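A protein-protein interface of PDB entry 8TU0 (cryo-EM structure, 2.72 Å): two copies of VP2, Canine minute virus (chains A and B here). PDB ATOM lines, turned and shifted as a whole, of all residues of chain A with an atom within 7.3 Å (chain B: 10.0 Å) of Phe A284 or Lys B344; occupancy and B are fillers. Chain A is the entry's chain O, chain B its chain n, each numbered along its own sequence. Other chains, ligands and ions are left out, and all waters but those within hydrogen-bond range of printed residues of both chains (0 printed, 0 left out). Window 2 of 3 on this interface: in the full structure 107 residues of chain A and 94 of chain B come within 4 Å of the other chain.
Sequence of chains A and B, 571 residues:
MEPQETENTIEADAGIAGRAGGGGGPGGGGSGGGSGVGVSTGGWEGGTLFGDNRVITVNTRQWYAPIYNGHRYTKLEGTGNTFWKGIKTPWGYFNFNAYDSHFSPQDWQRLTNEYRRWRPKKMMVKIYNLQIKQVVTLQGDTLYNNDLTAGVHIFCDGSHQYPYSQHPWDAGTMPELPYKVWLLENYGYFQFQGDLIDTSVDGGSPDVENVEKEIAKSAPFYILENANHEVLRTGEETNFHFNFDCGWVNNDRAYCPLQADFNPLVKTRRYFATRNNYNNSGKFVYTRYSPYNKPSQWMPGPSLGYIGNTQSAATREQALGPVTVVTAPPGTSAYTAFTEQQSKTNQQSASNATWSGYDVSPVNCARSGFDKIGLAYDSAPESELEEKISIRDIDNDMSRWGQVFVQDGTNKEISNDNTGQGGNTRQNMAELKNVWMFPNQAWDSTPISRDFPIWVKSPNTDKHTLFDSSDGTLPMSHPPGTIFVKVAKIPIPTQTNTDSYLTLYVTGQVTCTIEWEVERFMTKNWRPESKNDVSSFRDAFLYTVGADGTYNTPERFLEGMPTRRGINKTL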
ATOM      1  N   PHE A 272       0.150  -6.543 -14.212  1.00  0.00           N
ATOM      2  CA  PHE A 272      -1.142  -6.856 -14.805  1.00  0.00           C
ATOM      3  C   PHE A 272      -1.099  -6.655 -16.311  1.00  0.00           C
ATOM      4  O   PHE A 272      -0.454  -5.731 -16.810  1.00  0.00           O
ATOM      5  CB  PHE A 272      -2.279  -6.036 -14.193  1.00  0.00           C
ATOM      6  CG  PHE A 272      -2.155  -4.559 -14.382  1.00  0.00           C
ATOM      7  CD1 PHE A 272      -2.685  -3.943 -15.491  1.00  0.00           C
ATOM      8  CD2 PHE A 272      -1.558  -3.779 -13.420  1.00  0.00           C
ATOM      9  CE1 PHE A 272      -2.590  -2.589 -15.651  1.00  0.00           C
ATOM     10  CE2 PHE A 272      -1.460  -2.425 -13.578  1.00  0.00           C
ATOM     11  CZ  PHE A 272      -1.983  -1.830 -14.690  1.00  0.00           C
ATOM     12  N   ALA A 273      -1.789  -7.536 -17.021  1.00  0.00           N
ATOM     13  CA  ALA A 273      -1.739  -7.560 -18.470  1.00  0.00           C
ATOM     14  C   ALA A 273      -2.660  -6.513 -19.071  1.00  0.00           C
ATOM     15  O   ALA A 273      -3.706  -6.177 -18.514  1.00  0.00           O
ATOM     16  CB  ALA A 273      -2.126  -8.939 -18.990  1.00  0.00           C
ATOM     17  N   THR A 274      -2.250  -5.989 -20.221  1.00  0.00           N
ATOM     18  CA  THR A 274      -3.054  -5.044 -20.981  1.00  0.00           C
ATOM     19  C   THR A 274      -2.917  -5.357 -22.459  1.00  0.00           C
ATOM     20  O   THR A 274      -1.801  -5.389 -22.983  1.00  0.00           O
ATOM     21  CB  THR A 274      -2.615  -3.610 -20.707  1.00  0.00           C
ATOM     22  OG1 THR A 274      -2.886  -3.280 -19.342  1.00  0.00           O
ATOM     23  CG2 THR A 274      -3.339  -2.662 -21.616  1.00  0.00           C
ATOM     24  N   ARG A 275      -4.059  -5.481 -23.128  1.00  0.00           N
ATOM     25  CA  ARG A 275      -4.117  -5.700 -24.562  1.00  0.00           C
ATOM     26  C   ARG A 275      -3.781  -4.352 -25.169  1.00  0.00           C
ATOM     27  O   ARG A 275      -4.188  -3.325 -24.644  1.00  0.00           O
ATOM     28  CB  ARG A 275      -5.530  -6.075 -24.965  1.00  0.00           C
ATOM     29  CG  ARG A 275      -5.643  -6.668 -26.351  1.00  0.00           C
ATOM     30  CD  ARG A 275      -5.589  -8.172 -26.256  1.00  0.00           C
ATOM     31  NE  ARG A 275      -5.533  -8.792 -27.568  1.00  0.00           N
ATOM     32  CZ  ARG A 275      -6.537  -8.805 -28.426  1.00  0.00           C
ATOM     33  NH1 ARG A 275      -6.393  -9.406 -29.592  1.00  0.00           N
ATOM     34  NH2 ARG A 275      -7.679  -8.212 -28.121  1.00  0.00           N
ATOM     35  N   ASN A 276      -3.090  -4.332 -26.298  1.00  0.00           N
ATOM     36  CA  ASN A 276      -2.687  -3.051 -26.865  1.00  0.00           C
ATOM     37  C   ASN A 276      -3.504  -2.625 -28.084  1.00  0.00           C
ATOM     38  O   ASN A 276      -4.186  -1.598 -28.033  1.00  0.00           O
ATOM     39  CB  ASN A 276      -1.184  -3.090 -27.163  1.00  0.00           C
ATOM     40  CG  ASN A 276      -0.762  -4.357 -27.849  1.00  0.00           C
ATOM     41  OD1 ASN A 276      -1.504  -5.332 -27.868  1.00  0.00           O
ATOM     42  ND2 ASN A 276       0.445  -4.365 -28.393  1.00  0.00           N
ATOM     43  N   ASN A 279      -6.667  -6.019 -31.947  1.00  0.00           N
ATOM     44  CA  ASN A 279      -6.830  -6.851 -33.134  1.00  0.00           C
ATOM     45  C   ASN A 279      -6.076  -8.155 -32.927  1.00  0.00           C
ATOM     46  O   ASN A 279      -5.592  -8.443 -31.830  1.00  0.00           O
ATOM     47  CB  ASN A 279      -6.391  -6.090 -34.386  1.00  0.00           C
ATOM     48  CG  ASN A 279      -4.932  -5.719 -34.368  1.00  0.00           C
ATOM     49  OD1 ASN A 279      -4.078  -6.500 -33.956  1.00  0.00           O
ATOM     50  ND2 ASN A 279      -4.635  -4.502 -34.793  1.00  0.00           N
ATOM     51  N   ASN A 280      -5.971  -8.952 -33.991  1.00  0.00           N
ATOM     52  CA  ASN A 280      -5.313 -10.247 -33.865  1.00  0.00           C
ATOM     53  C   ASN A 280      -3.826 -10.102 -33.600  1.00  0.00           C
ATOM     54  O   ASN A 280      -3.233 -10.953 -32.933  1.00  0.00           O
ATOM     55  CB  ASN A 280      -5.528 -11.082 -35.119  1.00  0.00           C
ATOM     56  CG  ASN A 280      -6.957 -11.502 -35.293  1.00  0.00           C
ATOM     57  OD1 ASN A 280      -7.739 -11.476 -34.352  1.00  0.00           O
ATOM     58  ND2 ASN A 280      -7.302 -11.925 -36.494  1.00  0.00           N
ATOM     59  N   SER A 281      -3.204  -9.043 -34.113  1.00  0.00           N
ATOM     60  CA  SER A 281      -1.775  -8.856 -33.912  1.00  0.00           C
ATOM     61  C   SER A 281      -1.432  -8.444 -32.492  1.00  0.00           C
ATOM     62  O   SER A 281      -0.245  -8.363 -32.163  1.00  0.00           O
ATOM     63  CB  SER A 281      -1.244  -7.818 -34.894  1.00  0.00           C
ATOM     64  OG  SER A 281      -1.850  -6.560 -34.674  1.00  0.00           O
ATOM     65  N   GLY A 282      -2.426  -8.186 -31.655  1.00  0.00           N
ATOM     66  CA  GLY A 282      -2.174  -7.715 -30.313  1.00  0.00           C
ATOM     67  C   GLY A 282      -1.609  -8.776 -29.400  1.00  0.00           C
ATOM     68  O   GLY A 282      -1.561  -9.966 -29.706  1.00  0.00           O
ATOM     69  N   LYS A 283      -1.155  -8.305 -28.245  1.00  0.00           N
ATOM     70  CA  LYS A 283      -0.568  -9.138 -27.208  1.00  0.00           C
ATOM     71  C   LYS A 283      -0.682  -8.377 -25.901  1.00  0.00           C
ATOM     72  O   LYS A 283      -0.941  -7.175 -25.884  1.00  0.00           O
ATOM     73  CB  LYS A 283       0.888  -9.475 -27.512  1.00  0.00           C
ATOM     74  CG  LYS A 283       1.763  -8.254 -27.576  1.00  0.00           C
ATOM     75  CD  LYS A 283       3.163  -8.591 -28.019  1.00  0.00           C
ATOM     76  CE  LYS A 283       4.023  -7.343 -28.047  1.00  0.00           C
ATOM     77  NZ  LYS A 283       4.279  -6.816 -26.680  1.00  0.00           N
ATOM     78  N   PHE A 284      -0.485  -9.086 -24.801  1.00  0.00           N
ATOM     79  CA  PHE A 284      -0.579  -8.453 -23.496  1.00  0.00           C
ATOM     80  C   PHE A 284       0.726  -7.759 -23.143  1.00  0.00           C
ATOM     81  O   PHE A 284       1.803  -8.349 -23.241  1.00  0.00           O
ATOM     82  CB  PHE A 284      -0.941  -9.483 -22.434  1.00  0.00           C
ATOM     83  CG  PHE A 284      -2.280 -10.099 -22.640  1.00  0.00           C
ATOM     84  CD1 PHE A 284      -3.419  -9.439 -22.251  1.00  0.00           C
ATOM     85  CD2 PHE A 284      -2.400 -11.334 -23.228  1.00  0.00           C
ATOM     86  CE1 PHE A 284      -4.651  -9.995 -22.444  1.00  0.00           C
ATOM     87  CE2 PHE A 284      -3.634 -11.893 -23.420  1.00  0.00           C
ATOM     88  CZ  PHE A 284      -4.759 -11.222 -23.026  1.00  0.00           C
ATOM     89  N   VAL A 285       0.620  -6.498 -22.741  1.00  0.00           N
ATOM     90  CA  VAL A 285       1.745  -5.718 -22.250  1.00  0.00           C
ATOM     91  C   VAL A 285       1.562  -5.561 -20.752  1.00  0.00           C
ATOM     92  O   VAL A 285       0.457  -5.279 -20.283  1.00  0.00           O
ATOM     93  CB  VAL A 285       1.831  -4.350 -22.948  1.00  0.00           C
ATOM     94  CG1 VAL A 285       2.997  -3.556 -22.410  1.00  0.00           C
ATOM     95  CG2 VAL A 285       1.950  -4.538 -24.440  1.00  0.00           C
ATOM     96  N   TYR A 286       2.639  -5.747 -20.002  1.00  0.00           N
ATOM     97  CA  TYR A 286       2.559  -5.903 -18.561  1.00  0.00           C
ATOM     98  C   TYR A 286       3.114  -4.685 -17.845  1.00  0.00           C
ATOM     99  O   TYR A 286       4.138  -4.129 -18.247  1.00  0.00           O
ATOM    100  CB  TYR A 286       3.310  -7.152 -18.124  1.00  0.00           C
ATOM    101  CG  TYR A 286       2.691  -8.396 -18.677  1.00  0.00           C
ATOM    102  CD1 TYR A 286       1.680  -9.045 -18.000  1.00  0.00           C
ATOM    103  CD2 TYR A 286       3.099  -8.908 -19.891  1.00  0.00           C
ATOM    104  CE1 TYR A 286       1.108 -10.174 -18.505  1.00  0.00           C
ATOM    105  CE2 TYR A 286       2.526 -10.033 -20.407  1.00  0.00           C
ATOM    106  CZ  TYR A 286       1.529 -10.664 -19.710  1.00  0.00           C
ATOM    107  OH  TYR A 286       0.955 -11.802 -20.221  1.00  0.00           O
ATOM    108  N   GLY A 409     -12.274  -8.625 -19.995  1.00  0.00           N
ATOM    109  CA  GLY A 409     -11.396  -8.325 -21.112  1.00  0.00           C
ATOM    110  C   GLY A 409     -11.524  -6.879 -21.542  1.00  0.00           C
ATOM    111  O   GLY A 409     -11.882  -6.013 -20.754  1.00  0.00           O
ATOM    112  N   PRO B 329      -3.122 -28.628 -22.146  1.00  0.00           N
ATOM    113  CA  PRO B 329      -2.199 -27.750 -21.459  1.00  0.00           C
ATOM    114  C   PRO B 329      -2.076 -26.431 -22.194  1.00  0.00           C
ATOM    115  O   PRO B 329      -2.493 -26.327 -23.356  1.00  0.00           O
ATOM    116  CB  PRO B 329      -0.891 -28.546 -21.484  1.00  0.00           C
ATOM    117  CG  PRO B 329      -1.347 -29.953 -21.489  1.00  0.00           C
ATOM    118  CD  PRO B 329      -2.527 -29.949 -22.395  1.00  0.00           C
ATOM    119  N   PRO B 330      -1.525 -25.401 -21.548  1.00  0.00           N
ATOM    120  CA  PRO B 330      -1.631 -24.046 -22.114  1.00  0.00           C
ATOM    121  C   PRO B 330      -1.110 -23.900 -23.533  1.00  0.00           C
ATOM    122  O   PRO B 330      -1.786 -23.288 -24.369  1.00  0.00           O
ATOM    123  CB  PRO B 330      -0.823 -23.208 -21.120  1.00  0.00           C
ATOM    124  CG  PRO B 330      -0.962 -23.927 -19.850  1.00  0.00           C
ATOM    125  CD  PRO B 330      -0.960 -25.377 -20.192  1.00  0.00           C
ATOM    126  N   GLY B 331       0.062 -24.436 -23.841  1.00  0.00           N
ATOM    127  CA  GLY B 331       0.590 -24.207 -25.172  1.00  0.00           C
ATOM    128  C   GLY B 331       0.045 -25.109 -26.254  1.00  0.00           C
ATOM    129  O   GLY B 331       0.334 -24.890 -27.431  1.00  0.00           O
ATOM    130  N   THR B 332      -0.733 -26.118 -25.886  1.00  0.00           N
ATOM    131  CA  THR B 332      -1.144 -27.156 -26.814  1.00  0.00           C
ATOM    132  C   THR B 332      -2.298 -26.696 -27.702  1.00  0.00           C
ATOM    133  O   THR B 332      -3.068 -25.799 -27.357  1.00  0.00           O
ATOM    134  CB  THR B 332      -1.553 -28.407 -26.048  1.00  0.00           C
ATOM    135  OG1 THR B 332      -2.618 -28.080 -25.151  1.00  0.00           O
ATOM    136  CG2 THR B 332      -0.393 -28.924 -25.250  1.00  0.00           C
ATOM    137  N   PHE B 338      -8.545 -22.569 -32.254  1.00  0.00           N
ATOM    138  CA  PHE B 338      -8.264 -21.191 -32.600  1.00  0.00           C
ATOM    139  C   PHE B 338      -7.932 -20.444 -31.323  1.00  0.00           C
ATOM    140  O   PHE B 338      -8.185 -20.929 -30.219  1.00  0.00           O
ATOM    141  CB  PHE B 338      -9.457 -20.549 -33.306  1.00  0.00           C
ATOM    142  CG  PHE B 338     -10.718 -20.596 -32.504  1.00  0.00           C
ATOM    143  CD1 PHE B 338     -11.047 -19.571 -31.641  1.00  0.00           C
ATOM    144  CD2 PHE B 338     -11.565 -21.679 -32.596  1.00  0.00           C
ATOM    145  CE1 PHE B 338     -12.201 -19.622 -30.894  1.00  0.00           C
ATOM    146  CE2 PHE B 338     -12.721 -21.734 -31.852  1.00  0.00           C
ATOM    147  CZ  PHE B 338     -13.039 -20.704 -31.000  1.00  0.00           C
ATOM    148  N   THR B 339      -7.353 -19.261 -31.471  1.00  0.00           N
ATOM    149  CA  THR B 339      -7.031 -18.427 -30.324  1.00  0.00           C
ATOM    150  C   THR B 339      -8.173 -17.454 -30.074  1.00  0.00           C
ATOM    151  O   THR B 339      -8.491 -16.633 -30.939  1.00  0.00           O
ATOM    152  CB  THR B 339      -5.733 -17.657 -30.548  1.00  0.00           C
ATOM    153  OG1 THR B 339      -5.887 -16.798 -31.678  1.00  0.00           O
ATOM    154  CG2 THR B 339      -4.594 -18.613 -30.804  1.00  0.00           C
ATOM    155  N   GLU B 340      -8.791 -17.551 -28.901  1.00  0.00           N
ATOM    156  CA  GLU B 340      -9.675 -16.487 -28.459  1.00  0.00           C
ATOM    157  C   GLU B 340      -8.872 -15.206 -28.353  1.00  0.00           C
ATOM    158  O   GLU B 340      -7.847 -15.166 -27.677  1.00  0.00           O
ATOM    159  CB  GLU B 340     -10.286 -16.818 -27.104  1.00  0.00           C
ATOM    160  CG  GLU B 340     -11.273 -15.775 -26.632  1.00  0.00           C
ATOM    161  CD  GLU B 340     -11.785 -16.037 -25.233  1.00  0.00           C
ATOM    162  OE1 GLU B 340     -11.280 -16.969 -24.578  1.00  0.00           O
ATOM    163  OE2 GLU B 340     -12.701 -15.314 -24.789  1.00  0.00           O
ATOM    164  N   GLN B 341      -9.329 -14.153 -29.016  1.00  0.00           N
ATOM    165  CA  GLN B 341      -8.490 -12.968 -29.058  1.00  0.00           C
ATOM    166  C   GLN B 341      -8.556 -12.149 -27.781  1.00  0.00           C
ATOM    167  O   GLN B 341      -7.675 -11.317 -27.554  1.00  0.00           O
ATOM    168  CB  GLN B 341      -8.851 -12.108 -30.260  1.00  0.00           C
ATOM    169  CG  GLN B 341      -8.520 -12.773 -31.568  1.00  0.00           C
ATOM    170  CD  GLN B 341      -7.066 -13.176 -31.653  1.00  0.00           C
ATOM    171  OE1 GLN B 341      -6.186 -12.484 -31.151  1.00  0.00           O
ATOM    172  NE2 GLN B 341      -6.806 -14.299 -32.302  1.00  0.00           N
ATOM    173  N   GLN B 342      -9.561 -12.361 -26.939  1.00  0.00           N
ATOM    174  CA  GLN B 342      -9.564 -11.688 -25.649  1.00  0.00           C
ATOM    175  C   GLN B 342      -8.431 -12.197 -24.769  1.00  0.00           C
ATOM    176  O   GLN B 342      -7.593 -11.419 -24.305  1.00  0.00           O
ATOM    177  CB  GLN B 342     -10.911 -11.875 -24.961  1.00  0.00           C
ATOM    178  CG  GLN B 342     -12.031 -11.141 -25.641  1.00  0.00           C
ATOM    179  CD  GLN B 342     -11.822  -9.649 -25.618  1.00  0.00           C
ATOM    180  OE1 GLN B 342     -11.444  -9.053 -26.615  1.00  0.00           O
ATOM    181  NE2 GLN B 342     -12.045  -9.041 -24.470  1.00  0.00           N
ATOM    182  N   SER B 343      -8.387 -13.504 -24.533  1.00  0.00           N
ATOM    183  CA  SER B 343      -7.367 -14.085 -23.676  1.00  0.00           C
ATOM    184  C   SER B 343      -6.137 -14.559 -24.431  1.00  0.00           C
ATOM    185  O   SER B 343      -5.120 -14.851 -23.796  1.00  0.00           O
ATOM    186  CB  SER B 343      -7.958 -15.255 -22.896  1.00  0.00           C
ATOM    187  OG  SER B 343      -8.363 -16.282 -23.774  1.00  0.00           O
ATOM    188  N   LYS B 344      -6.195 -14.619 -25.756  1.00  0.00           N
ATOM    189  CA  LYS B 344      -5.107 -15.141 -26.579  1.00  0.00           C
ATOM    190  C   LYS B 344      -4.671 -16.523 -26.104  1.00  0.00           C
ATOM    191  O   LYS B 344      -3.494 -16.787 -25.860  1.00  0.00           O
ATOM    192  CB  LYS B 344      -3.933 -14.175 -26.620  1.00  0.00           C
ATOM    193  CG  LYS B 344      -4.283 -12.878 -27.295  1.00  0.00           C
ATOM    194  CD  LYS B 344      -3.054 -12.078 -27.547  1.00  0.00           C
ATOM    195  CE  LYS B 344      -2.244 -12.766 -28.623  1.00  0.00           C
ATOM    196  NZ  LYS B 344      -2.989 -12.761 -29.907  1.00  0.00           N
ATOM    197  N   THR B 345      -5.648 -17.413 -25.972  1.00  0.00           N
ATOM    198  CA  THR B 345      -5.406 -18.803 -25.631  1.00  0.00           C
ATOM    199  C   THR B 345      -6.130 -19.691 -26.627  1.00  0.00           C
ATOM    200  O   THR B 345      -7.183 -19.329 -27.152  1.00  0.00           O
ATOM    201  CB  THR B 345      -5.882 -19.138 -24.220  1.00  0.00           C
ATOM    202  OG1 THR B 345      -7.270 -18.815 -24.100  1.00  0.00           O
ATOM    203  CG2 THR B 345      -5.090 -18.361 -23.185  1.00  0.00           C
ATOM    204  N   ASN B 346      -5.555 -20.857 -26.884  1.00  0.00           N
ATOM    205  CA  ASN B 346      -6.176 -21.794 -27.804  1.00  0.00           C
ATOM    206  C   ASN B 346      -7.473 -22.318 -27.218  1.00  0.00           C
ATOM    207  O   ASN B 346      -7.509 -22.789 -26.079  1.00  0.00           O
ATOM    208  CB  ASN B 346      -5.230 -22.945 -28.109  1.00  0.00           C
ATOM    209  CG  ASN B 346      -4.085 -22.525 -28.983  1.00  0.00           C
ATOM    210  OD1 ASN B 346      -4.240 -22.366 -30.190  1.00  0.00           O
ATOM    211  ND2 ASN B 346      -2.923 -22.331 -28.381  1.00  0.00           N
ATOM    212  N   GLN B 347      -8.542 -22.228 -27.996  1.00  0.00           N
ATOM    213  CA  GLN B 347      -9.835 -22.734 -27.581  1.00  0.00           C
ATOM    214  C   GLN B 347     -10.474 -23.452 -28.752  1.00  0.00           C
ATOM    215  O   GLN B 347     -10.032 -23.339 -29.895  1.00  0.00           O
ATOM    216  CB  GLN B 347     -10.740 -21.616 -27.075  1.00  0.00           C
ATOM    217  CG  GLN B 347     -10.267 -20.972 -25.794  1.00  0.00           C
ATOM    218  CD  GLN B 347     -11.225 -19.920 -25.311  1.00  0.00           C
ATOM    219  OE1 GLN B 347     -11.970 -19.341 -26.098  1.00  0.00           O
ATOM    220  NE2 GLN B 347     -11.237 -19.682 -24.006  1.00  0.00           N
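No position is printed for both chains. Of the 9 pairs that touch across the chains among the printed residues, none has its exchanged pair printed and touching as well.
Of chain B, only Gln B342 (3.1 Å), Ser B343 (3.3 Å) and Lys B344 (3.9 Å) come within 4 Å of Phe A284. Of chain A, only Asn A280, Gly A282, Lys A283 and Phe A284 come within 4 Å of Lys B344. No residue of chain B comes within 4 Å of Ala A273. No residue of chain B comes within 4 Å of Val A285. Of the printed residues of chain B, Arg A275 touches Gln B341. Of the printed residues of chain A, Gln B341 touches Arg A275 and Asn A280. Of the printed residues of chain B, Asn A280 touches Gln B341 and Lys B344. Of the printed residues of chain A, Gln B342 touches Phe A284 (3.1 Å) and Gly A409 (3.5 Å). The nearest residue of chain B that does not touch Phe A284 is Gln B341 (5.4 Å). The nearest printed residue of chain B that does not touch Arg A275 is Lys B344 (4.1 Å).
Gln B341 touches Asn A280 (CG to OD1, 3.2 Å). Asn A280 touches Lys B344. Lys A283 touches Lys B344 (CA to CD, 3.9 Å). CZ of Phe A284 touches O of Gln B342, at 3.1 Å. Ser B343 touches Phe A284. Lys B344 touches Phe A284 (CB to CE2, 3.9 Å). CA of Gly A409 touches NE2 of Gln B342 (3.5 Å).
NH1 of Arg A275 lies close to O of Gln B341, 3.1 Å away. The backbone carbonyl oxygen of Gly A282 sits close to the side-chain amino group of Lys B344 (3.1 Å).
The guanidinium group (NH1) of Arg A275 sits at hydrogen-bond distance from the backbone carbonyl oxygen (O) of Asn A279 (2.6 Å). The side-chain amide oxygen of Asn A276 sits close to the backbone carbonyl oxygen of Lys A283 (2.8 Å). OE1 of Glu B340 lies within hydrogen-bond range of OG of Ser B343. The side-chain amide oxygen (OE1) of Gln B341 sits at hydrogen-bond distance from the side-chain amino group (NZ) of Lys B344, 3.4 Å away. The backbone NH of Gly A282 is in hydrogen-bond range of the side-chain amide oxygen of Asn A279. The side-chain hydroxyl (OG) of Ser B343 lies within hydrogen-bond range of the side-chain hydroxyl (OG1) of Thr B345.
Of the 14 printed residues of chain A, 6 touch a printed residue of chain B. Among the printed residues, 9 pairs touch across the chains.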
